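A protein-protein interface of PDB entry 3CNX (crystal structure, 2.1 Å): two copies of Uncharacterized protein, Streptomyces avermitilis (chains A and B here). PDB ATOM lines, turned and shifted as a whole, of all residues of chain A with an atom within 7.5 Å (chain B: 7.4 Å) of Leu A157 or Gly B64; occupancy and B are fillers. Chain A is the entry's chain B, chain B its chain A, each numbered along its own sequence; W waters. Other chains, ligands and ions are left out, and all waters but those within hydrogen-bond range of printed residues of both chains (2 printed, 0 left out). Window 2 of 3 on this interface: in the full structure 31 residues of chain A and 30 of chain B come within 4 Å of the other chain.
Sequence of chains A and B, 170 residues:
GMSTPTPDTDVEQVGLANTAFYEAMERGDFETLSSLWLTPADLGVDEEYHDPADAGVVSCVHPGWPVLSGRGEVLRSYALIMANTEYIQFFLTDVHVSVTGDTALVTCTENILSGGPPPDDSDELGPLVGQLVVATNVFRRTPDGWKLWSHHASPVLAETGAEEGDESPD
The backbone NH (N) of Leu A157 sits at hydrogen-bond distance from the backbone carbonyl oxygen (O) of Gly B64 (2.8 Å). NE2 of His B152 is in hydrogen-bond range of OG of Ser A154, at 2.8 Å.
O of Val B61 is in hydrogen-bond range of N of Ala B153 (2.8 Å). The backbone carbonyl oxygen of Leu A132 lies within hydrogen-bond range of the backbone NH of Val A156 (3.0 Å). The backbone carbonyl oxygen of Ser A154 lies within hydrogen-bond range of the backbone NH of Val A134 (3.0 Å).
Among the printed residues, pairs that only touch across the chains: Val A156 with Gly B64 (3.5 Å), Pro A155 with Gly B64 (3.5 Å), Ser A154 with Ser B154 (3.7 Å), Val A134 with Trp B65 (3.7 Å), Ser A154 with Val B61 (3.8 Å), Val A134 with His B152 (3.9 Å) and Val A156 with Trp B65 (3.97 Å).
Leu A157 touches just one residue of chain B: Gly B64 (2.8 Å). Of the printed residues of chain A, Gly B64 touches Pro A155, Val A156 and Leu A157. Printed residues of chain A within 4 Å of Trp B65: Val A134 and Val A156. Printed residues of chain B within 4 Å of Val A156: Gly B64 (3.5 Å) and Trp B65 (3.97 Å). Of the printed residues of chain A, His B152 touches Val A134 and Ser A154. Of the printed residues of chain B, Pro A155 touches Gly B64 (3.5 Å). Ala B153 touches none of the printed residues of chain A. Leu B157 touches none of the printed residues of chain A.
Hydrophobic or aromatic side chains of chain B within 4 Å of the printed part of chain A: Val B61 and His B152. Printed residues of chain A that touch a printed residue of chain B: Val A134, Ser A154, Pro A155, Val A156 and Leu A157. Hydrophobic or aromatic side chains of chain A that line the printed part of chain B: Val A134, Val A156 and Leu A157. Among the printed residues, 9 pairs touch across the chains. Among the printed residues, no Asp or Glu carboxylate lies within 4 Å of a Lys or Arg side-chain nitrogen of the other chain.
Ser B154 touches its own counterpart, Ser A154. Positions printed for both chains: 154, 155 and 157.
Water W1 lies within hydrogen-bond range of O of Ala B153 (2.7 Å), N of Gly B64 (2.8 Å), O of His B62 (3.3 Å) and OG of Ser A154 (3.3 Å). Water W2 lies within hydrogen-bond range of the backbone carbonyl oxygen of Pro A155 (2.7 Å), the side-chain hydroxyl of Ser A154 (2.8 Å) and the backbone carbonyl oxygen of Trp B65 (3.0 Å).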
ATOM      1  N   LEU A 132       9.467 -24.606  33.640  1.00  0.00           N
ATOM      2  CA  LEU A 132       8.172 -25.075  33.152  1.00  0.00           C
ATOM      3  C   LEU A 132       7.854 -24.269  31.909  1.00  0.00           C
ATOM      4  O   LEU A 132       7.683 -23.053  31.954  1.00  0.00           O
ATOM      5  CB  LEU A 132       7.081 -24.876  34.191  1.00  0.00           C
ATOM      6  CG  LEU A 132       5.725 -25.483  33.845  1.00  0.00           C
ATOM      7  CD1 LEU A 132       5.837 -26.993  33.820  1.00  0.00           C
ATOM      8  CD2 LEU A 132       4.639 -25.030  34.841  1.00  0.00           C
ATOM      9  N   VAL A 134       5.922 -24.810  27.857  1.00  0.00           N
ATOM     10  CA  VAL A 134       5.057 -25.571  26.963  1.00  0.00           C
ATOM     11  C   VAL A 134       5.458 -25.251  25.501  1.00  0.00           C
ATOM     12  O   VAL A 134       5.987 -24.184  25.216  1.00  0.00           O
ATOM     13  CB  VAL A 134       3.566 -25.277  27.211  1.00  0.00           C
ATOM     14  CG1 VAL A 134       3.156 -25.714  28.602  1.00  0.00           C
ATOM     15  CG2 VAL A 134       3.248 -23.799  27.010  1.00  0.00           C
ATOM     16  N   SER A 154       7.469 -21.603  25.173  1.00  0.00           N
ATOM     17  CA  SER A 154       7.184 -20.463  26.035  1.00  0.00           C
ATOM     18  C   SER A 154       7.100 -20.833  27.514  1.00  0.00           C
ATOM     19  O   SER A 154       6.690 -21.950  27.844  1.00  0.00           O
ATOM     20  CB  SER A 154       5.869 -19.796  25.581  1.00  0.00           C
ATOM     21  OG  SER A 154       4.824 -20.746  25.483  1.00  0.00           O
ATOM     22  N   PRO A 155       7.524 -19.917  28.408  1.00  0.00           N
ATOM     23  CA  PRO A 155       7.356 -20.126  29.823  1.00  0.00           C
ATOM     24  C   PRO A 155       5.909 -20.138  30.246  1.00  0.00           C
ATOM     25  O   PRO A 155       5.075 -19.418  29.733  1.00  0.00           O
ATOM     26  CB  PRO A 155       8.105 -18.934  30.446  1.00  0.00           C
ATOM     27  CG  PRO A 155       7.980 -17.872  29.451  1.00  0.00           C
ATOM     28  CD  PRO A 155       8.130 -18.595  28.147  1.00  0.00           C
ATOM     29  N   VAL A 156       5.616 -20.995  31.191  1.00  0.00           N
ATOM     30  CA  VAL A 156       4.341 -20.916  31.886  1.00  0.00           C
ATOM     31  C   VAL A 156       4.589 -20.032  33.089  1.00  0.00           C
ATOM     32  O   VAL A 156       5.337 -20.407  33.974  1.00  0.00           O
ATOM     33  CB  VAL A 156       3.858 -22.309  32.324  1.00  0.00           C
ATOM     34  CG1 VAL A 156       2.589 -22.222  33.188  1.00  0.00           C
ATOM     35  CG2 VAL A 156       3.639 -23.161  31.099  1.00  0.00           C
ATOM     36  N   LEU A 157       3.992 -18.840  33.069  1.00  0.00           N
ATOM     37  CA  LEU A 157       4.247 -17.782  34.064  1.00  0.00           C
ATOM     38  C   LEU A 157       3.159 -17.620  35.139  1.00  0.00           C
ATOM     39  O   LEU A 157       1.963 -17.583  34.843  1.00  0.00           O
ATOM     40  CB  LEU A 157       4.407 -16.445  33.351  1.00  0.00           C
ATOM     41  CG  LEU A 157       5.613 -16.331  32.430  1.00  0.00           C
ATOM     42  CD1 LEU A 157       5.602 -14.966  31.710  1.00  0.00           C
ATOM     43  CD2 LEU A 157       6.899 -16.539  33.175  1.00  0.00           C
ATOM     44  N   ALA A 158       3.590 -17.513  36.392  1.00  0.00           N
ATOM     45  CA  ALA A 158       2.640 -17.297  37.510  1.00  0.00           C
ATOM     46  C   ALA A 158       2.018 -15.894  37.454  1.00  0.00           C
ATOM     47  O   ALA A 158       0.873 -15.707  37.901  1.00  0.00           O
ATOM     48  CB  ALA A 158       3.296 -17.543  38.890  1.00  0.00           C
ATOM     49  N   VAL B  61      -2.132 -21.330  23.022  1.00  0.00           N
ATOM     50  CA  VAL B  61      -1.305 -20.828  24.118  1.00  0.00           C
ATOM     51  C   VAL B  61      -1.376 -19.328  24.085  1.00  0.00           C
ATOM     52  O   VAL B  61      -1.020 -18.670  23.111  1.00  0.00           O
ATOM     53  CB  VAL B  61       0.174 -21.356  24.087  1.00  0.00           C
ATOM     54  CG1 VAL B  61       0.994 -20.852  25.291  1.00  0.00           C
ATOM     55  CG2 VAL B  61       0.182 -22.862  24.039  1.00  0.00           C
ATOM     56  N   HIS B  62      -1.954 -18.822  25.159  1.00  0.00           N
ATOM     57  CA  HIS B  62      -1.958 -17.424  25.453  1.00  0.00           C
ATOM     58  C   HIS B  62      -0.673 -17.072  26.169  1.00  0.00           C
ATOM     59  O   HIS B  62      -0.036 -17.915  26.787  1.00  0.00           O
ATOM     60  CB  HIS B  62      -3.152 -17.012  26.337  1.00  0.00           C
ATOM     61  CG  HIS B  62      -4.481 -17.279  25.719  1.00  0.00           C
ATOM     62  ND1 HIS B  62      -4.852 -16.759  24.503  1.00  0.00           N
ATOM     63  CD2 HIS B  62      -5.542 -17.989  26.168  1.00  0.00           C
ATOM     64  CE1 HIS B  62      -6.078 -17.161  24.218  1.00  0.00           C
ATOM     65  NE2 HIS B  62      -6.513 -17.926  25.205  1.00  0.00           N
ATOM     66  N   PRO B  63      -0.289 -15.814  26.090  1.00  0.00           N
ATOM     67  CA  PRO B  63       0.973 -15.376  26.658  1.00  0.00           C
ATOM     68  C   PRO B  63       1.144 -15.759  28.143  1.00  0.00           C
ATOM     69  O   PRO B  63       0.396 -15.302  28.995  1.00  0.00           O
ATOM     70  CB  PRO B  63       0.908 -13.847  26.457  1.00  0.00           C
ATOM     71  CG  PRO B  63       0.057 -13.671  25.236  1.00  0.00           C
ATOM     72  CD  PRO B  63      -1.015 -14.701  25.432  1.00  0.00           C
ATOM     73  N   GLY B  64       2.126 -16.623  28.419  1.00  0.00           N
ATOM     74  CA  GLY B  64       2.411 -17.085  29.776  1.00  0.00           C
ATOM     75  C   GLY B  64       1.531 -18.204  30.309  1.00  0.00           C
ATOM     76  O   GLY B  64       1.684 -18.637  31.455  1.00  0.00           O
ATOM     77  N   TRP B  65       0.636 -18.675  29.455  1.00  0.00           N
ATOM     78  CA  TRP B  65      -0.337 -19.732  29.818  1.00  0.00           C
ATOM     79  C   TRP B  65       0.097 -21.156  29.569  1.00  0.00           C
ATOM     80  O   TRP B  65       0.975 -21.409  28.738  1.00  0.00           O
ATOM     81  CB  TRP B  65      -1.624 -19.528  29.039  1.00  0.00           C
ATOM     82  CG  TRP B  65      -2.512 -18.431  29.563  1.00  0.00           C
ATOM     83  CD1 TRP B  65      -2.148 -17.184  29.890  1.00  0.00           C
ATOM     84  CD2 TRP B  65      -3.929 -18.521  29.796  1.00  0.00           C
ATOM     85  NE1 TRP B  65      -3.241 -16.471  30.310  1.00  0.00           N
ATOM     86  CE2 TRP B  65      -4.352 -17.274  30.248  1.00  0.00           C
ATOM     87  CE3 TRP B  65      -4.872 -19.530  29.629  1.00  0.00           C
ATOM     88  CZ2 TRP B  65      -5.696 -17.004  30.577  1.00  0.00           C
ATOM     89  CZ3 TRP B  65      -6.207 -19.268  29.952  1.00  0.00           C
ATOM     90  CH2 TRP B  65      -6.603 -18.017  30.425  1.00  0.00           C
ATOM     91  N   PRO B  66      -0.524 -22.129  30.286  1.00  0.00           N
ATOM     92  CA  PRO B  66      -0.287 -23.459  29.791  1.00  0.00           C
ATOM     93  C   PRO B  66      -1.120 -23.654  28.542  1.00  0.00           C
ATOM     94  O   PRO B  66      -1.728 -22.677  28.011  1.00  0.00           O
ATOM     95  CB  PRO B  66      -0.782 -24.378  30.917  1.00  0.00           C
ATOM     96  CG  PRO B  66      -1.694 -23.562  31.729  1.00  0.00           C
ATOM     97  CD  PRO B  66      -1.627 -22.108  31.250  1.00  0.00           C
ATOM     98  N   VAL B 133       4.470  -9.278  22.069  1.00  0.00           N
ATOM     99  CA  VAL B 133       4.176 -10.698  22.042  1.00  0.00           C
ATOM    100  C   VAL B 133       4.549 -11.152  20.647  1.00  0.00           C
ATOM    101  O   VAL B 133       4.616 -10.340  19.731  1.00  0.00           O
ATOM    102  CB  VAL B 133       2.688 -10.942  22.482  1.00  0.00           C
ATOM    103  CG1 VAL B 133       2.140 -12.289  21.990  1.00  0.00           C
ATOM    104  CG2 VAL B 133       2.601 -10.841  24.016  1.00  0.00           C
ATOM    105  N   HIS B 152      -0.265 -19.900  19.049  1.00  0.00           N
ATOM    106  CA  HIS B 152       0.702 -19.900  20.138  1.00  0.00           C
ATOM    107  C   HIS B 152       1.348 -18.560  20.256  1.00  0.00           C
ATOM    108  O   HIS B 152       2.017 -18.151  19.358  1.00  0.00           O
ATOM    109  CB  HIS B 152       1.762 -21.011  19.908  1.00  0.00           C
ATOM    110  CG  HIS B 152       2.566 -21.348  21.128  1.00  0.00           C
ATOM    111  ND1 HIS B 152       2.913 -22.651  21.473  1.00  0.00           N
ATOM    112  CD2 HIS B 152       3.058 -20.555  22.105  1.00  0.00           C
ATOM    113  CE1 HIS B 152       3.591 -22.618  22.610  1.00  0.00           C
ATOM    114  NE2 HIS B 152       3.723 -21.357  22.989  1.00  0.00           N
ATOM    115  N   ALA B 153       1.107 -17.894  21.387  1.00  0.00           N
ATOM    116  CA  ALA B 153       1.536 -16.530  21.621  1.00  0.00           C
ATOM    117  C   ALA B 153       2.357 -16.467  22.874  1.00  0.00           C
ATOM    118  O   ALA B 153       2.100 -17.159  23.843  1.00  0.00           O
ATOM    119  CB  ALA B 153       0.315 -15.538  21.709  1.00  0.00           C
ATOM    120  N   SER B 154       3.410 -15.672  22.811  1.00  0.00           N
ATOM    121  CA  SER B 154       4.366 -15.629  23.892  1.00  0.00           C
ATOM    122  C   SER B 154       4.983 -14.265  24.060  1.00  0.00           C
ATOM    123  O   SER B 154       5.141 -13.563  23.095  1.00  0.00           O
ATOM    124  CB  SER B 154       5.480 -16.677  23.680  1.00  0.00           C
ATOM    125  OG  SER B 154       6.093 -16.625  22.398  1.00  0.00           O
ATOM    126  N   PRO B 155       5.320 -13.897  25.293  1.00  0.00           N
ATOM    127  CA  PRO B 155       6.037 -12.666  25.577  1.00  0.00           C
ATOM    128  C   PRO B 155       7.488 -12.721  25.109  1.00  0.00           C
ATOM    129  O   PRO B 155       8.129 -13.762  25.176  1.00  0.00           O
ATOM    130  CB  PRO B 155       5.994 -12.580  27.112  1.00  0.00           C
ATOM    131  CG  PRO B 155       5.897 -13.967  27.566  1.00  0.00           C
ATOM    132  CD  PRO B 155       5.085 -14.684  26.514  1.00  0.00           C
ATOM    133  N   LEU B 157      10.740 -11.542  26.270  1.00  0.00           N
ATOM    134  CA  LEU B 157      11.270 -11.144  27.581  1.00  0.00           C
ATOM    135  C   LEU B 157      12.717 -10.690  27.513  1.00  0.00           C
ATOM    136  O   LEU B 157      13.545 -11.315  26.862  1.00  0.00           O
ATOM    137  CB  LEU B 157      11.122 -12.293  28.581  1.00  0.00           C
ATOM    138  CG  LEU B 157       9.685 -12.765  28.823  1.00  0.00           C
ATOM    139  CD1 LEU B 157       9.648 -13.987  29.689  1.00  0.00           C
ATOM    140  CD2 LEU B 157       8.833 -11.654  29.419  1.00  0.00           C
HETATM  141  O   HOH W   1       3.225 -17.884  26.158  1.00  0.00           O
HETATM  142  O   HOH W   2       3.339 -19.938  27.761  1.00  0.00           O
